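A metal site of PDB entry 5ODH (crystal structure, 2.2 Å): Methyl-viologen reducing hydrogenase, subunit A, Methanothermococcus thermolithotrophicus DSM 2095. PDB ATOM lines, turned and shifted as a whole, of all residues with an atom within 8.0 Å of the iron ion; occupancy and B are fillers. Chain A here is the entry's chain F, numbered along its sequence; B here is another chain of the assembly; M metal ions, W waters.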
ATOM      1  N   GLU A  42     -20.302   1.636  -1.731  1.00  0.00           N
ATOM      2  CA  GLU A  42     -19.881   0.771  -2.835  1.00  0.00           C
ATOM      3  C   GLU A  42     -19.575  -0.633  -2.366  1.00  0.00           C
ATOM      4  O   GLU A  42     -19.801  -1.601  -3.102  1.00  0.00           O
ATOM      5  CB  GLU A  42     -18.679   1.390  -3.546  1.00  0.00           C
ATOM      6  CG  GLU A  42     -19.077   2.540  -4.480  1.00  0.00           C
ATOM      7  CD  GLU A  42     -17.977   3.554  -4.682  1.00  0.00           C
ATOM      8  OE1 GLU A  42     -17.100   3.683  -3.813  1.00  0.00           O
ATOM      9  OE2 GLU A  42     -17.997   4.231  -5.740  1.00  0.00           O
ATOM     10  N   GLU A 264     -10.424   8.150 -11.296  1.00  0.00           N
ATOM     11  CA  GLU A 264     -10.505   8.870 -10.025  1.00  0.00           C
ATOM     12  C   GLU A 264      -9.231   8.626  -9.229  1.00  0.00           C
ATOM     13  O   GLU A 264      -8.903   7.484  -8.908  1.00  0.00           O
ATOM     14  CB  GLU A 264     -11.741   8.429  -9.234  1.00  0.00           C
ATOM     15  CG  GLU A 264     -12.984   8.205 -10.079  1.00  0.00           C
ATOM     16  CD  GLU A 264     -14.223   7.918  -9.235  1.00  0.00           C
ATOM     17  OE1 GLU A 264     -14.608   8.786  -8.424  1.00  0.00           O
ATOM     18  OE2 GLU A 264     -14.798   6.820  -9.367  1.00  0.00           O
ATOM     19  N   LEU A 272     -12.472  12.628  -0.338  1.00  0.00           N
ATOM     20  CA  LEU A 272     -13.033  12.831  -1.660  1.00  0.00           C
ATOM     21  C   LEU A 272     -11.953  12.601  -2.705  1.00  0.00           C
ATOM     22  O   LEU A 272     -10.827  13.075  -2.558  1.00  0.00           O
ATOM     23  CB  LEU A 272     -13.626  14.238  -1.791  1.00  0.00           C
ATOM     24  CG  LEU A 272     -14.538  14.448  -3.016  1.00  0.00           C
ATOM     25  CD1 LEU A 272     -15.406  13.221  -3.265  1.00  0.00           C
ATOM     26  CD2 LEU A 272     -15.414  15.684  -2.848  1.00  0.00           C
ATOM     27  N   LYS A 273     -12.303  11.832  -3.734  1.00  0.00           N
ATOM     28  CA  LYS A 273     -11.360  11.484  -4.787  1.00  0.00           C
ATOM     29  C   LYS A 273     -11.242  12.643  -5.790  1.00  0.00           C
ATOM     30  O   LYS A 273     -11.965  13.639  -5.721  1.00  0.00           O
ATOM     31  CB  LYS A 273     -11.791  10.186  -5.470  1.00  0.00           C
ATOM     32  CG  LYS A 273     -11.405   8.930  -4.668  1.00  0.00           C
ATOM     33  CD  LYS A 273     -12.500   7.876  -4.667  1.00  0.00           C
ATOM     34  CE  LYS A 273     -12.636   7.194  -6.009  1.00  0.00           C
ATOM     35  NZ  LYS A 273     -13.642   6.094  -5.965  1.00  0.00           N
ATOM     36  N   ILE A 379     -23.363   8.234 -12.061  1.00  0.00           N
ATOM     37  CA  ILE A 379     -23.235   6.917 -12.669  1.00  0.00           C
ATOM     38  C   ILE A 379     -23.340   5.862 -11.571  1.00  0.00           C
ATOM     39  O   ILE A 379     -22.588   5.897 -10.584  1.00  0.00           O
ATOM     40  CB  ILE A 379     -21.912   6.767 -13.443  1.00  0.00           C
ATOM     41  CG1 ILE A 379     -21.909   7.717 -14.650  1.00  0.00           C
ATOM     42  CG2 ILE A 379     -21.714   5.320 -13.902  1.00  0.00           C
ATOM     43  CD1 ILE A 379     -20.553   7.882 -15.289  1.00  0.00           C
ATOM     44  N   THR A 393     -19.987  -2.995  -7.108  1.00  0.00           N
ATOM     45  CA  THR A 393     -20.604  -1.727  -7.461  1.00  0.00           C
ATOM     46  C   THR A 393     -19.545  -0.645  -7.564  1.00  0.00           C
ATOM     47  O   THR A 393     -18.559  -0.643  -6.825  1.00  0.00           O
ATOM     48  CB  THR A 393     -21.650  -1.260  -6.443  1.00  0.00           C
ATOM     49  OG1 THR A 393     -20.992  -0.765  -5.266  1.00  0.00           O
ATOM     50  CG2 THR A 393     -22.584  -2.391  -6.051  1.00  0.00           C
ATOM     51  N   ASN A 394     -19.791   0.312  -8.468  1.00  0.00           N
ATOM     52  CA  ASN A 394     -18.994   1.531  -8.537  1.00  0.00           C
ATOM     53  C   ASN A 394     -19.921   2.714  -8.754  1.00  0.00           C
ATOM     54  O   ASN A 394     -20.822   2.659  -9.599  1.00  0.00           O
ATOM     55  CB  ASN A 394     -17.948   1.452  -9.660  1.00  0.00           C
ATOM     56  CG  ASN A 394     -17.119   2.725  -9.786  1.00  0.00           C
ATOM     57  OD1 ASN A 394     -16.687   3.294  -8.787  1.00  0.00           O
ATOM     58  ND2 ASN A 394     -16.884   3.159 -11.018  1.00  0.00           N
ATOM     59  N   LEU A 395     -19.675   3.801  -8.017  1.00  0.00           N
ATOM     60  CA  LEU A 395     -20.514   4.994  -8.063  1.00  0.00           C
ATOM     61  C   LEU A 395     -19.626   6.194  -8.348  1.00  0.00           C
ATOM     62  O   LEU A 395     -18.740   6.510  -7.544  1.00  0.00           O
ATOM     63  CB  LEU A 395     -21.260   5.205  -6.746  1.00  0.00           C
ATOM     64  CG  LEU A 395     -22.075   4.031  -6.180  1.00  0.00           C
ATOM     65  CD1 LEU A 395     -22.690   4.402  -4.826  1.00  0.00           C
ATOM     66  CD2 LEU A 395     -23.166   3.606  -7.153  1.00  0.00           C
ATOM     67  N   VAL A 396     -19.844   6.846  -9.493  1.00  0.00           N
ATOM     68  CA  VAL A 396     -19.215   8.119  -9.821  1.00  0.00           C
ATOM     69  C   VAL A 396     -20.287   9.185  -9.599  1.00  0.00           C
ATOM     70  O   VAL A 396     -21.186   9.352 -10.430  1.00  0.00           O
ATOM     71  CB  VAL A 396     -18.668   8.142 -11.254  1.00  0.00           C
ATOM     72  CG1 VAL A 396     -17.975   9.462 -11.529  1.00  0.00           C
ATOM     73  CG2 VAL A 396     -17.722   6.977 -11.479  1.00  0.00           C
ATOM     74  N   VAL A 397     -20.187   9.901  -8.481  1.00  0.00           N
ATOM     75  CA  VAL A 397     -21.296  10.701  -7.987  1.00  0.00           C
ATOM     76  C   VAL A 397     -20.931  12.169  -8.116  1.00  0.00           C
ATOM     77  O   VAL A 397     -20.241  12.737  -7.256  1.00  0.00           O
ATOM     78  CB  VAL A 397     -21.667  10.340  -6.539  1.00  0.00           C
ATOM     79  CG1 VAL A 397     -22.851  11.167  -6.075  1.00  0.00           C
ATOM     80  CG2 VAL A 397     -21.972   8.856  -6.427  1.00  0.00           C
ATOM     81  N   VAL A 400     -17.981  14.707  -6.814  1.00  0.00           N
ATOM     82  CA  VAL A 400     -16.603  14.227  -6.776  1.00  0.00           C
ATOM     83  C   VAL A 400     -15.816  14.804  -7.944  1.00  0.00           C
ATOM     84  O   VAL A 400     -14.621  15.110  -7.805  1.00  0.00           O
ATOM     85  CB  VAL A 400     -16.560  12.675  -6.781  1.00  0.00           C
ATOM     86  CG1 VAL A 400     -17.134  12.117  -8.064  1.00  0.00           C
ATOM     87  CG2 VAL A 400     -15.126  12.177  -6.580  1.00  0.00           C
ATOM     88  N   CYS A 445     -22.755  12.996  -0.881  1.00  0.00           N
ATOM     89  CA  CYS A 445     -22.887  12.365  -2.189  1.00  0.00           C
ATOM     90  C   CYS A 445     -21.524  12.097  -2.824  1.00  0.00           C
ATOM     91  O   CYS A 445     -21.300  11.033  -3.406  1.00  0.00           O
ATOM     92  CB  CYS A 445     -23.705  13.254  -3.106  1.00  0.00           C
ATOM     93  SG  CYS A 445     -25.197  12.474  -3.646  1.00  0.00           S
ATOM     94  N   ALA A 446     -20.616  13.071  -2.739  1.00  0.00           N
ATOM     95  CA  ALA A 446     -19.333  12.949  -3.421  1.00  0.00           C
ATOM     96  C   ALA A 446     -18.517  11.781  -2.891  1.00  0.00           C
ATOM     97  O   ALA A 446     -17.775  11.144  -3.649  1.00  0.00           O
ATOM     98  CB  ALA A 446     -18.577  14.262  -3.284  1.00  0.00           C
ATOM     99  N   THR A 447     -18.633  11.480  -1.590  1.00  0.00           N
ATOM    100  CA  THR A 447     -17.858  10.400  -0.976  1.00  0.00           C
ATOM    101  C   THR A 447     -18.611   9.074  -0.962  1.00  0.00           C
ATOM    102  O   THR A 447     -17.993   8.022  -1.148  1.00  0.00           O
ATOM    103  CB  THR A 447     -17.471  10.781   0.453  1.00  0.00           C
ATOM    104  OG1 THR A 447     -18.646  11.157   1.194  1.00  0.00           O
ATOM    105  CG2 THR A 447     -16.475  11.934   0.445  1.00  0.00           C
ATOM    106  N   HIS A 448     -19.921   9.107  -0.719  1.00  0.00           N
ATOM    107  CA  HIS A 448     -20.753   7.905  -0.566  1.00  0.00           C
ATOM    108  C   HIS A 448     -20.042   6.767   0.169  1.00  0.00           C
ATOM    109  O   HIS A 448     -19.618   6.921   1.318  1.00  0.00           O
ATOM    110  CB  HIS A 448     -21.249   7.416  -1.936  1.00  0.00           C
ATOM    111  CG  HIS A 448     -20.220   7.461  -3.023  1.00  0.00           C
ATOM    112  ND1 HIS A 448     -19.984   8.590  -3.781  1.00  0.00           N
ATOM    113  CD2 HIS A 448     -19.358   6.524  -3.492  1.00  0.00           C
ATOM    114  CE1 HIS A 448     -19.035   8.350  -4.659  1.00  0.00           C
ATOM    115  NE2 HIS A 448     -18.640   7.093  -4.512  1.00  0.00           N
ATOM    116  N   LYS B 106     -12.332  -0.708  -1.016  1.00  0.00           N
ATOM    117  CA  LYS B 106     -13.235  -0.677  -2.166  1.00  0.00           C
ATOM    118  C   LYS B 106     -13.350   0.747  -2.712  1.00  0.00           C
ATOM    119  O   LYS B 106     -13.202   0.969  -3.908  1.00  0.00           O
ATOM    120  CB  LYS B 106     -14.606  -1.223  -1.765  1.00  0.00           C
ATOM    121  CG  LYS B 106     -15.696  -1.100  -2.848  1.00  0.00           C
ATOM    122  CD  LYS B 106     -15.266  -1.685  -4.185  1.00  0.00           C
ATOM    123  CE  LYS B 106     -15.028  -3.181  -4.096  1.00  0.00           C
ATOM    124  NZ  LYS B 106     -14.651  -3.760  -5.410  1.00  0.00           N
ATOM    125  N   ALA B 107     -13.602   1.716  -1.820  1.00  0.00           N
ATOM    126  CA  ALA B 107     -13.822   3.084  -2.274  1.00  0.00           C
ATOM    127  C   ALA B 107     -12.565   3.702  -2.873  1.00  0.00           C
ATOM    128  O   ALA B 107     -12.671   4.514  -3.798  1.00  0.00           O
ATOM    129  CB  ALA B 107     -14.304   3.937  -1.101  1.00  0.00           C
ATOM    130  N   TYR B 108     -11.379   3.322  -2.381  1.00  0.00           N
ATOM    131  CA  TYR B 108     -10.155   4.035  -2.732  1.00  0.00           C
ATOM    132  C   TYR B 108      -9.094   3.152  -3.374  1.00  0.00           C
ATOM    133  O   TYR B 108      -7.948   3.601  -3.517  1.00  0.00           O
ATOM    134  CB  TYR B 108      -9.588   4.713  -1.480  1.00  0.00           C
ATOM    135  CG  TYR B 108     -10.603   5.623  -0.833  1.00  0.00           C
ATOM    136  CD1 TYR B 108     -11.027   6.780  -1.467  1.00  0.00           C
ATOM    137  CD2 TYR B 108     -11.141   5.318   0.406  1.00  0.00           C
ATOM    138  CE1 TYR B 108     -11.960   7.618  -0.890  1.00  0.00           C
ATOM    139  CE2 TYR B 108     -12.072   6.147   0.998  1.00  0.00           C
ATOM    140  CZ  TYR B 108     -12.486   7.292   0.347  1.00  0.00           C
ATOM    141  OH  TYR B 108     -13.411   8.120   0.931  1.00  0.00           O
ATOM    142  N   THR B 111     -12.403  -0.029  -6.705  1.00  0.00           N
ATOM    143  CA  THR B 111     -13.455   0.451  -7.605  1.00  0.00           C
ATOM    144  C   THR B 111     -12.850   0.672  -8.996  1.00  0.00           C
ATOM    145  O   THR B 111     -11.709   1.112  -9.117  1.00  0.00           O
ATOM    146  CB  THR B 111     -14.090   1.741  -7.079  1.00  0.00           C
ATOM    147  OG1 THR B 111     -13.152   2.473  -6.296  1.00  0.00           O
ATOM    148  CG2 THR B 111     -15.310   1.422  -6.230  1.00  0.00           C
ATOM    149  N   ILE B 112     -13.632   0.355 -10.035  1.00  0.00           N
ATOM    150  CA  ILE B 112     -13.053   0.139 -11.358  1.00  0.00           C
ATOM    151  C   ILE B 112     -12.418   1.422 -11.903  1.00  0.00           C
ATOM    152  O   ILE B 112     -11.387   1.374 -12.586  1.00  0.00           O
ATOM    153  CB  ILE B 112     -14.109  -0.439 -12.326  1.00  0.00           C
ATOM    154  CG1 ILE B 112     -15.268   0.524 -12.546  1.00  0.00           C
ATOM    155  CG2 ILE B 112     -14.629  -1.774 -11.793  1.00  0.00           C
ATOM    156  CD1 ILE B 112     -16.024   0.234 -13.826  1.00  0.00           C
ATOM    157  N   THR B 113     -13.032   2.578 -11.628  1.00  0.00           N
ATOM    158  CA  THR B 113     -12.481   3.830 -12.143  1.00  0.00           C
ATOM    159  C   THR B 113     -11.403   4.394 -11.243  1.00  0.00           C
ATOM    160  O   THR B 113     -10.761   5.382 -11.615  1.00  0.00           O
ATOM    161  CB  THR B 113     -13.580   4.880 -12.318  1.00  0.00           C
ATOM    162  OG1 THR B 113     -14.367   4.969 -11.126  1.00  0.00           O
ATOM    163  CG2 THR B 113     -14.465   4.546 -13.524  1.00  0.00           C
ATOM    164  N   THR B 114     -11.173   3.813 -10.074  1.00  0.00           N
ATOM    165  CA  THR B 114     -10.195   4.356  -9.156  1.00  0.00           C
ATOM    166  C   THR B 114      -8.791   4.080  -9.675  1.00  0.00           C
ATOM    167  O   THR B 114      -8.495   2.984 -10.154  1.00  0.00           O
ATOM    168  CB  THR B 114     -10.368   3.763  -7.765  1.00  0.00           C
ATOM    169  OG1 THR B 114     -11.707   4.000  -7.306  1.00  0.00           O
ATOM    170  CG2 THR B 114      -9.406   4.392  -6.782  1.00  0.00           C
HETATM  171 FE    FE M   1     -17.252   6.161  -5.985  1.00  0.00          FE
HETATM  172  O   HOH W   1     -15.956   5.817  -4.465  1.00  0.00           O
HETATM  173  O   HOH W   2     -15.766   5.109  -7.451  1.00  0.00           O
HETATM  174  O   HOH W   3     -16.397   8.173  -6.396  1.00  0.00           O
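OD1 of Asn 394 sits close to OE2 of Glu 42, 3.4 Å away.
The backbone carbonyl oxygen (O) of Glu 42 is in hydrogen-bond range of the side-chain hydroxyl (OG1) of Thr 393 (2.6 Å).
The backbone carbonyl oxygen (O) of Ala 446 lies close to a ring nitrogen (ND1) of His 448 (3.4 Å).
A ring nitrogen (ND1) of His 448 is in hydrogen-bond range of the backbone carbonyl oxygen (O) of Cys 445.
OE2 of Glu 264 lies within salt-bridge range of NZ of Lys 273 (3.7 Å).
O of Ala 107 of chain B is in hydrogen-bond range of NZ of Lys 273 (2.9 Å).
The side-chain hydroxyl of Thr 114 of chain B is in hydrogen-bond range of the side-chain amino group of Lys 273 (3.2 Å).
Lys 273 touches the iron ion (NZ to FE, 3.6 Å).
Of the 22 residues printed, 4 come within 4 Å of the iron ion.
The iron ion is bound by water W1 (2.0 Å), the side-chain carboxylate of Glu 42 (2.1 Å), the backbone carbonyl oxygen of Leu 395 (2.2 Å), water W3 (2.2 Å), a ring nitrogen (NE2) of His 448 (2.2 Å) and water W2 (2.3 Å).
The iron ion has six donor atoms within binding distance.
Water W1 lies within hydrogen-bond range of the side-chain carboxylate of Glu 42 and the side-chain amino group of Lys 273.
Water W2 lies within hydrogen-bond range of OD1 of Asn 394 (2.4 Å), OE2 of Glu 264 (2.7 Å) and NZ of Lys 273 (2.8 Å).
Water W3 bridges the side-chain carboxylate (OE1) of Glu 264 (2.8 Å) and the side-chain amino group (NZ) of Lys 273 (3.5 Å).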
